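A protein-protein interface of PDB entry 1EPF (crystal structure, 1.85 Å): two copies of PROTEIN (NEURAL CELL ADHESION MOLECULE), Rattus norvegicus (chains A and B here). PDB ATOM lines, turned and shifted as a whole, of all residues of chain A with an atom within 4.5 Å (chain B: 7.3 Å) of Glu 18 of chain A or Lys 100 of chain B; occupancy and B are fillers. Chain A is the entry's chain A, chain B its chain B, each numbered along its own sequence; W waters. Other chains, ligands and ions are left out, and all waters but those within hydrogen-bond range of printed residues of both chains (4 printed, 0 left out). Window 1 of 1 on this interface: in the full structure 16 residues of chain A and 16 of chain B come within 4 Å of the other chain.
The side-chain carboxylate of Glu 18 of chain A lies within salt-bridge range of the side-chain amino group of Lys 100 of chain B.
The side-chain hydroxyl of Ser 19 of chain A sits at hydrogen-bond distance from the backbone NH of Asn 68 of chain A, 3.2 Å away. The backbone NH of Ala 69 of chain A lies within hydrogen-bond range of the backbone carbonyl oxygen of Glu 18 of chain A. The backbone NH (N) of Asn 68 of chain A sits at hydrogen-bond distance from the backbone carbonyl oxygen (O) of Glu 18 of chain A.
Among the printed residues, pairs that only touch across the chains: Ser 19 of chain A with Ile 182 of chain B (3.8 Å) and Tyr 67 of chain A with Ile 182 of chain B (3.6 Å).
Printed residues of chain A within 4 Å of Lys 100 of chain B: Glu 18. No residue of chain B comes within 4 Å of Gly 17 of chain A. Of the printed residues of chain B, Ser 19 of chain A touches Ile 182. Of the printed residues of chain B, Tyr 67 of chain A touches Ile 182 (3.6 Å). Of the printed residues of chain A, Ile 182 of chain B touches Ser 19 (3.8 Å) and Tyr 67 (3.6 Å). Ser 127 of chain B touches none of the printed residues of chain A. The nearest printed residue of chain A that does not touch Lys 100 of chain B is Ser 15 of chain A (5.9 Å). The nearest printed residue of chain B that does not touch Ser 19 of chain A is Glu 181 of chain B (4.5 Å).
Hydrophobic or aromatic side chains of chain B within 4 Å of the printed part of chain A: Ile 182. Along chain A the printed residues that touch a printed residue of chain B span positions 18 to 67. Among the printed residues, 3 pairs touch across the chains. Among the printed residues, Asp or Glu carboxylates within 4 Å of a Lys or Arg side-chain nitrogen of the other chain: Glu 18 of chain A with Lys 100 of chain B (2.5 Å).
Positions printed for both chains: 15, 16 and 18. Of the 3 pairs that touch across the chains among the printed residues, none has its exchanged pair printed and touching as well.
Water W1 lies within hydrogen-bond range of the side-chain carboxylate of Glu 18 of chain A (2.4 Å) and the side-chain amino group of Lys 100 of chain B (3.3 Å). Water W2 bridges the backbone carbonyl oxygen (O) of Ser 19 of chain A (2.5 Å) and the backbone NH (N) of Ile 182 of chain B (3.2 Å). Water W3 lies within hydrogen-bond range of OE1 of Glu 18 of chain A (2.6 Å), NZ of Lys 100 of chain B (3.2 Å) and OG of Ser 15 of chain A (3.2 Å). Water W4 bridges the backbone carbonyl oxygen (O) of Ile 182 of chain B (2.8 Å) and the backbone NH (N) of Ser 19 of chain A (3.0 Å).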
ATOM      1  N   ILE A  14     -23.035 -14.411   3.796  1.00  0.00           N
ATOM      2  CA  ILE A  14     -23.675 -15.438   4.609  1.00  0.00           C
ATOM      3  C   ILE A  14     -22.592 -16.255   5.306  1.00  0.00           C
ATOM      4  O   ILE A  14     -21.635 -16.697   4.670  1.00  0.00           O
ATOM      5  CB  ILE A  14     -24.514 -16.415   3.756  1.00  0.00           C
ATOM      6  CG1 ILE A  14     -25.378 -15.645   2.751  1.00  0.00           C
ATOM      7  CG2 ILE A  14     -25.391 -17.268   4.673  1.00  0.00           C
ATOM      8  CD1 ILE A  14     -26.157 -16.547   1.799  1.00  0.00           C
ATOM      9  N   SER A  15     -22.737 -16.442   6.612  1.00  0.00           N
ATOM     10  CA  SER A  15     -21.774 -17.227   7.366  1.00  0.00           C
ATOM     11  C   SER A  15     -22.041 -18.680   7.011  1.00  0.00           C
ATOM     12  O   SER A  15     -23.187 -19.063   6.797  1.00  0.00           O
ATOM     13  CB  SER A  15     -21.963 -17.028   8.870  1.00  0.00           C
ATOM     14  OG  SER A  15     -21.590 -15.725   9.269  1.00  0.00           O
ATOM     15  N   VAL A  16     -20.983 -19.484   6.938  1.00  0.00           N
ATOM     16  CA  VAL A  16     -21.124 -20.898   6.614  1.00  0.00           C
ATOM     17  C   VAL A  16     -22.110 -21.535   7.588  1.00  0.00           C
ATOM     18  O   VAL A  16     -22.026 -21.322   8.795  1.00  0.00           O
ATOM     19  CB  VAL A  16     -19.757 -21.628   6.714  1.00  0.00           C
ATOM     20  CG1 VAL A  16     -19.937 -23.130   6.502  1.00  0.00           C
ATOM     21  CG2 VAL A  16     -18.795 -21.063   5.685  1.00  0.00           C
ATOM     22  N   GLY A  17     -23.058 -22.295   7.055  1.00  0.00           N
ATOM     23  CA  GLY A  17     -24.034 -22.954   7.902  1.00  0.00           C
ATOM     24  C   GLY A  17     -25.236 -22.107   8.281  1.00  0.00           C
ATOM     25  O   GLY A  17     -26.160 -22.593   8.937  1.00  0.00           O
ATOM     26  N   GLU A  18     -25.242 -20.841   7.880  1.00  0.00           N
ATOM     27  CA  GLU A  18     -26.368 -19.976   8.204  1.00  0.00           C
ATOM     28  C   GLU A  18     -27.172 -19.655   6.957  1.00  0.00           C
ATOM     29  O   GLU A  18     -26.846 -20.125   5.867  1.00  0.00           O
ATOM     30  CB  GLU A  18     -25.882 -18.710   8.911  1.00  0.00           C
ATOM     31  CG  GLU A  18     -25.614 -18.951  10.394  1.00  0.00           C
ATOM     32  CD  GLU A  18     -24.871 -17.818  11.051  1.00  0.00           C
ATOM     33  OE1 GLU A  18     -25.232 -16.645  10.817  1.00  0.00           O
ATOM     34  OE2 GLU A  18     -23.926 -18.104  11.811  1.00  0.00           O
ATOM     35  N   SER A  19     -28.216 -18.853   7.110  1.00  0.00           N
ATOM     36  CA  SER A  19     -29.075 -18.549   5.981  1.00  0.00           C
ATOM     37  C   SER A  19     -29.327 -17.069   5.740  1.00  0.00           C
ATOM     38  O   SER A  19     -29.240 -16.256   6.655  1.00  0.00           O
ATOM     39  CB  SER A  19     -30.407 -19.272   6.186  1.00  0.00           C
ATOM     40  OG  SER A  19     -30.182 -20.609   6.591  1.00  0.00           O
ATOM     41  N   ILE A  66     -31.158 -18.730   0.699  1.00  0.00           N
ATOM     42  CA  ILE A  66     -30.087 -19.711   0.733  1.00  0.00           C
ATOM     43  C   ILE A  66     -29.958 -20.167   2.183  1.00  0.00           C
ATOM     44  O   ILE A  66     -29.519 -19.400   3.034  1.00  0.00           O
ATOM     45  CB  ILE A  66     -28.741 -19.105   0.287  1.00  0.00           C
ATOM     46  CG1 ILE A  66     -28.828 -18.652  -1.175  1.00  0.00           C
ATOM     47  CG2 ILE A  66     -27.629 -20.132   0.475  1.00  0.00           C
ATOM     48  CD1 ILE A  66     -27.580 -17.942  -1.670  1.00  0.00           C
ATOM     49  N   TYR A  67     -30.362 -21.408   2.453  1.00  0.00           N
ATOM     50  CA  TYR A  67     -30.296 -21.987   3.795  1.00  0.00           C
ATOM     51  C   TYR A  67     -29.024 -22.828   3.960  1.00  0.00           C
ATOM     52  O   TYR A  67     -28.492 -23.337   2.977  1.00  0.00           O
ATOM     53  CB  TYR A  67     -31.504 -22.898   4.046  1.00  0.00           C
ATOM     54  CG  TYR A  67     -32.842 -22.195   4.159  1.00  0.00           C
ATOM     55  CD1 TYR A  67     -33.230 -21.590   5.357  1.00  0.00           C
ATOM     56  CD2 TYR A  67     -33.727 -22.154   3.083  1.00  0.00           C
ATOM     57  CE1 TYR A  67     -34.469 -20.957   5.481  1.00  0.00           C
ATOM     58  CE2 TYR A  67     -34.978 -21.523   3.197  1.00  0.00           C
ATOM     59  CZ  TYR A  67     -35.335 -20.930   4.401  1.00  0.00           C
ATOM     60  OH  TYR A  67     -36.545 -20.295   4.538  1.00  0.00           O
ATOM     61  N   ASN A  68     -28.540 -22.957   5.198  1.00  0.00           N
ATOM     62  CA  ASN A  68     -27.357 -23.776   5.491  1.00  0.00           C
ATOM     63  C   ASN A  68     -26.279 -23.563   4.420  1.00  0.00           C
ATOM     64  O   ASN A  68     -25.805 -24.506   3.782  1.00  0.00           O
ATOM     65  CB  ASN A  68     -27.780 -25.251   5.526  1.00  0.00           C
ATOM     66  CG  ASN A  68     -26.652 -26.180   5.930  1.00  0.00           C
ATOM     67  OD1 ASN A  68     -26.749 -27.398   5.767  1.00  0.00           O
ATOM     68  ND2 ASN A  68     -25.582 -25.617   6.468  1.00  0.00           N
ATOM     69  N   ALA A  69     -25.896 -22.307   4.238  1.00  0.00           N
ATOM     70  CA  ALA A  69     -24.921 -21.929   3.230  1.00  0.00           C
ATOM     71  C   ALA A  69     -23.571 -22.626   3.302  1.00  0.00           C
ATOM     72  O   ALA A  69     -23.014 -22.835   4.378  1.00  0.00           O
ATOM     73  CB  ALA A  69     -24.718 -20.434   3.275  1.00  0.00           C
ATOM     74  N   SER B  15     -19.658 -10.375  18.239  1.00  0.00           N
ATOM     75  CA  SER B  15     -20.872 -11.184  18.176  1.00  0.00           C
ATOM     76  C   SER B  15     -20.899 -12.050  19.423  1.00  0.00           C
ATOM     77  O   SER B  15     -19.856 -12.532  19.867  1.00  0.00           O
ATOM     78  CB  SER B  15     -20.871 -12.080  16.936  1.00  0.00           C
ATOM     79  OG  SER B  15     -21.006 -11.317  15.748  1.00  0.00           O
ATOM     80  N   VAL B  16     -22.081 -12.241  19.995  1.00  0.00           N
ATOM     81  CA  VAL B  16     -22.206 -13.066  21.194  1.00  0.00           C
ATOM     82  C   VAL B  16     -21.480 -14.405  21.023  1.00  0.00           C
ATOM     83  O   VAL B  16     -21.652 -15.088  20.012  1.00  0.00           O
ATOM     84  CB  VAL B  16     -23.698 -13.336  21.525  1.00  0.00           C
ATOM     85  CG1 VAL B  16     -23.814 -14.272  22.724  1.00  0.00           C
ATOM     86  CG2 VAL B  16     -24.407 -12.023  21.807  1.00  0.00           C
ATOM     87  N   GLU B  18     -18.319 -14.899  20.512  1.00  0.00           N
ATOM     88  CA  GLU B  18     -17.063 -14.784  19.784  1.00  0.00           C
ATOM     89  C   GLU B  18     -16.099 -13.919  20.593  1.00  0.00           C
ATOM     90  O   GLU B  18     -16.459 -13.432  21.662  1.00  0.00           O
ATOM     91  CB  GLU B  18     -17.315 -14.230  18.375  1.00  0.00           C
ATOM     92  CG  GLU B  18     -17.938 -15.295  17.449  1.00  0.00           C
ATOM     93  CD  GLU B  18     -18.308 -14.770  16.074  1.00  0.00           C
ATOM     94  OE1 GLU B  18     -17.659 -13.828  15.582  1.00  0.00           O
ATOM     95  OE2 GLU B  18     -19.250 -15.323  15.467  1.00  0.00           O
ATOM     96  N   PHE B  98     -23.227  -7.845  19.582  1.00  0.00           N
ATOM     97  CA  PHE B  98     -24.280  -8.126  18.618  1.00  0.00           C
ATOM     98  C   PHE B  98     -24.834  -9.530  18.768  1.00  0.00           C
ATOM     99  O   PHE B  98     -24.093 -10.505  18.795  1.00  0.00           O
ATOM    100  CB  PHE B  98     -23.748  -7.938  17.192  1.00  0.00           C
ATOM    101  CG  PHE B  98     -24.704  -8.390  16.123  1.00  0.00           C
ATOM    102  CD1 PHE B  98     -25.802  -7.614  15.774  1.00  0.00           C
ATOM    103  CD2 PHE B  98     -24.498  -9.599  15.464  1.00  0.00           C
ATOM    104  CE1 PHE B  98     -26.686  -8.038  14.779  1.00  0.00           C
ATOM    105  CE2 PHE B  98     -25.371 -10.030  14.476  1.00  0.00           C
ATOM    106  CZ  PHE B  98     -26.467  -9.250  14.130  1.00  0.00           C
ATOM    107  N   GLN B  99     -26.152  -9.617  18.856  1.00  0.00           N
ATOM    108  CA  GLN B  99     -26.833 -10.891  18.991  1.00  0.00           C
ATOM    109  C   GLN B  99     -27.599 -11.159  17.705  1.00  0.00           C
ATOM    110  O   GLN B  99     -28.591 -10.485  17.421  1.00  0.00           O
ATOM    111  CB  GLN B  99     -27.805 -10.846  20.173  1.00  0.00           C
ATOM    112  CG  GLN B  99     -28.668 -12.088  20.307  1.00  0.00           C
ATOM    113  CD  GLN B  99     -27.838 -13.336  20.479  1.00  0.00           C
ATOM    114  OE1 GLN B  99     -27.293 -13.586  21.553  1.00  0.00           O
ATOM    115  NE2 GLN B  99     -27.718 -14.119  19.412  1.00  0.00           N
ATOM    116  N   LYS B 100     -27.129 -12.115  16.910  1.00  0.00           N
ATOM    117  CA  LYS B 100     -27.835 -12.439  15.680  1.00  0.00           C
ATOM    118  C   LYS B 100     -29.133 -13.141  16.082  1.00  0.00           C
ATOM    119  O   LYS B 100     -29.292 -13.554  17.232  1.00  0.00           O
ATOM    120  CB  LYS B 100     -26.993 -13.350  14.786  1.00  0.00           C
ATOM    121  CG  LYS B 100     -26.725 -14.728  15.348  1.00  0.00           C
ATOM    122  CD  LYS B 100     -25.812 -15.500  14.415  1.00  0.00           C
ATOM    123  CE  LYS B 100     -25.459 -16.864  14.977  1.00  0.00           C
ATOM    124  NZ  LYS B 100     -24.337 -17.478  14.221  1.00  0.00           N
ATOM    125  N   LEU B 101     -30.052 -13.278  15.134  1.00  0.00           N
ATOM    126  CA  LEU B 101     -31.340 -13.913  15.398  1.00  0.00           C
ATOM    127  C   LEU B 101     -31.195 -15.368  15.846  1.00  0.00           C
ATOM    128  O   LEU B 101     -30.729 -16.221  15.085  1.00  0.00           O
ATOM    129  CB  LEU B 101     -32.214 -13.841  14.143  1.00  0.00           C
ATOM    130  CG  LEU B 101     -33.696 -14.191  14.300  1.00  0.00           C
ATOM    131  CD1 LEU B 101     -34.310 -13.334  15.385  1.00  0.00           C
ATOM    132  CD2 LEU B 101     -34.411 -13.954  12.985  1.00  0.00           C
ATOM    133  N   MET B 102     -31.601 -15.645  17.082  1.00  0.00           N
ATOM    134  CA  MET B 102     -31.510 -16.994  17.633  1.00  0.00           C
ATOM    135  C   MET B 102     -32.735 -17.338  18.469  1.00  0.00           C
ATOM    136  O   MET B 102     -33.477 -16.456  18.895  1.00  0.00           O
ATOM    137  CB  MET B 102     -30.262 -17.128  18.508  1.00  0.00           C
ATOM    138  CG  MET B 102     -28.961 -16.916  17.765  1.00  0.00           C
ATOM    139  SD  MET B 102     -28.731 -18.118  16.437  1.00  0.00           S
ATOM    140  CE  MET B 102     -28.217 -19.553  17.353  1.00  0.00           C
ATOM    141  N   PHE B 103     -32.946 -18.629  18.696  1.00  0.00           N
ATOM    142  CA  PHE B 103     -34.077 -19.062  19.500  1.00  0.00           C
ATOM    143  C   PHE B 103     -33.609 -19.517  20.870  1.00  0.00           C
ATOM    144  O   PHE B 103     -33.015 -20.584  21.016  1.00  0.00           O
ATOM    145  CB  PHE B 103     -34.841 -20.183  18.794  1.00  0.00           C
ATOM    146  CG  PHE B 103     -35.337 -19.795  17.436  1.00  0.00           C
ATOM    147  CD1 PHE B 103     -34.498 -19.870  16.330  1.00  0.00           C
ATOM    148  CD2 PHE B 103     -36.624 -19.295  17.271  1.00  0.00           C
ATOM    149  CE1 PHE B 103     -34.934 -19.443  15.079  1.00  0.00           C
ATOM    150  CE2 PHE B 103     -37.068 -18.865  16.022  1.00  0.00           C
ATOM    151  CZ  PHE B 103     -36.221 -18.941  14.925  1.00  0.00           C
ATOM    152  N   VAL B 124     -37.387 -15.617  21.081  1.00  0.00           N
ATOM    153  CA  VAL B 124     -36.352 -15.191  20.143  1.00  0.00           C
ATOM    154  C   VAL B 124     -35.526 -14.034  20.698  1.00  0.00           C
ATOM    155  O   VAL B 124     -36.071 -13.128  21.321  1.00  0.00           O
ATOM    156  CB  VAL B 124     -36.990 -14.718  18.809  1.00  0.00           C
ATOM    157  CG1 VAL B 124     -35.918 -14.211  17.872  1.00  0.00           C
ATOM    158  CG2 VAL B 124     -37.769 -15.863  18.154  1.00  0.00           C
ATOM    159  N   VAL B 125     -34.216 -14.071  20.465  1.00  0.00           N
ATOM    160  CA  VAL B 125     -33.313 -13.005  20.894  1.00  0.00           C
ATOM    161  C   VAL B 125     -32.677 -12.484  19.617  1.00  0.00           C
ATOM    162  O   VAL B 125     -32.406 -13.254  18.696  1.00  0.00           O
ATOM    163  CB  VAL B 125     -32.212 -13.510  21.872  1.00  0.00           C
ATOM    164  CG1 VAL B 125     -32.817 -13.755  23.257  1.00  0.00           C
ATOM    165  CG2 VAL B 125     -31.590 -14.797  21.344  1.00  0.00           C
ATOM    166  N   SER B 126     -32.447 -11.180  19.566  1.00  0.00           N
ATOM    167  CA  SER B 126     -31.885 -10.558  18.382  1.00  0.00           C
ATOM    168  C   SER B 126     -31.684  -9.074  18.662  1.00  0.00           C
ATOM    169  O   SER B 126     -32.600  -8.406  19.152  1.00  0.00           O
ATOM    170  CB  SER B 126     -32.860 -10.770  17.210  1.00  0.00           C
ATOM    171  OG  SER B 126     -32.506 -10.032  16.051  1.00  0.00           O
ATOM    172  N   SER B 127     -30.488  -8.559  18.379  1.00  0.00           N
ATOM    173  CA  SER B 127     -30.219  -7.134  18.589  1.00  0.00           C
ATOM    174  C   SER B 127     -31.137  -6.284  17.712  1.00  0.00           C
ATOM    175  O   SER B 127     -31.581  -5.209  18.118  1.00  0.00           O
ATOM    176  CB  SER B 127     -28.757  -6.803  18.274  1.00  0.00           C
ATOM    177  OG  SER B 127     -27.891  -7.486  19.166  1.00  0.00           O
ATOM    178  N   LEU B 128     -31.427  -6.767  16.512  1.00  0.00           N
ATOM    179  CA  LEU B 128     -32.306  -6.047  15.590  1.00  0.00           C
ATOM    180  C   LEU B 128     -33.725  -6.620  15.686  1.00  0.00           C
ATOM    181  O   LEU B 128     -33.904  -7.832  15.761  1.00  0.00           O
ATOM    182  CB  LEU B 128     -31.779  -6.187  14.160  1.00  0.00           C
ATOM    183  CG  LEU B 128     -30.325  -5.755  13.936  1.00  0.00           C
ATOM    184  CD1 LEU B 128     -29.881  -6.172  12.548  1.00  0.00           C
ATOM    185  CD2 LEU B 128     -30.201  -4.245  14.122  1.00  0.00           C
ATOM    186  N   ILE B 176     -35.052 -10.423   9.322  1.00  0.00           N
ATOM    187  CA  ILE B 176     -34.667  -9.041   9.605  1.00  0.00           C
ATOM    188  C   ILE B 176     -34.827  -8.389   8.243  1.00  0.00           C
ATOM    189  O   ILE B 176     -33.958  -8.486   7.381  1.00  0.00           O
ATOM    190  CB  ILE B 176     -33.202  -8.905  10.095  1.00  0.00           C
ATOM    191  CG1 ILE B 176     -32.995  -9.719  11.377  1.00  0.00           C
ATOM    192  CG2 ILE B 176     -32.875  -7.430  10.356  1.00  0.00           C
ATOM    193  CD1 ILE B 176     -33.935  -9.355  12.518  1.00  0.00           C
ATOM    194  N   GLU B 181     -31.400 -11.338   6.908  1.00  0.00           N
ATOM    195  CA  GLU B 181     -31.188 -12.378   7.909  1.00  0.00           C
ATOM    196  C   GLU B 181     -32.472 -13.147   8.186  1.00  0.00           C
ATOM    197  O   GLU B 181     -33.548 -12.570   8.304  1.00  0.00           O
ATOM    198  CB  GLU B 181     -30.656 -11.820   9.240  1.00  0.00           C
ATOM    199  CG  GLU B 181     -30.565 -12.935  10.310  1.00  0.00           C
ATOM    200  CD  GLU B 181     -29.829 -12.537  11.579  1.00  0.00           C
ATOM    201  OE1 GLU B 181     -30.026 -11.401  12.043  1.00  0.00           O
ATOM    202  OE2 GLU B 181     -29.070 -13.374  12.122  1.00  0.00           O
ATOM    203  N   ILE B 182     -32.344 -14.459   8.287  1.00  0.00           N
ATOM    204  CA  ILE B 182     -33.493 -15.289   8.555  1.00  0.00           C
ATOM    205  C   ILE B 182     -33.047 -16.506   9.353  1.00  0.00           C
ATOM    206  O   ILE B 182     -31.931 -16.995   9.181  1.00  0.00           O
ATOM    207  CB  ILE B 182     -34.171 -15.726   7.221  1.00  0.00           C
ATOM    208  CG1 ILE B 182     -35.332 -16.681   7.505  1.00  0.00           C
ATOM    209  CG2 ILE B 182     -33.139 -16.375   6.290  1.00  0.00           C
ATOM    210  CD1 ILE B 182     -36.019 -17.210   6.250  1.00  0.00           C
ATOM    211  N   ASN B 183     -33.899 -16.962  10.261  1.00  0.00           N
ATOM    212  CA  ASN B 183     -33.613 -18.151  11.049  1.00  0.00           C
ATOM    213  C   ASN B 183     -34.975 -18.724  11.415  1.00  0.00           C
ATOM    214  O   ASN B 183     -35.975 -18.009  11.389  1.00  0.00           O
ATOM    215  CB  ASN B 183     -32.809 -17.807  12.311  1.00  0.00           C
ATOM    216  CG  ASN B 183     -32.019 -18.999  12.838  1.00  0.00           C
ATOM    217  OD1 ASN B 183     -32.167 -20.122  12.351  1.00  0.00           O
ATOM    218  ND2 ASN B 183     -31.179 -18.761  13.839  1.00  0.00           N
HETATM  219  O   HOH W   1     -21.984 -19.264  12.683  1.00  0.00           O
HETATM  220  O   HOH W   2     -29.115 -14.654   8.580  1.00  0.00           O
HETATM  221  O   HOH W   3     -23.292 -15.447  12.011  1.00  0.00           O
HETATM  222  O   HOH W   4     -29.411 -18.096   9.735  1.00  0.00           O
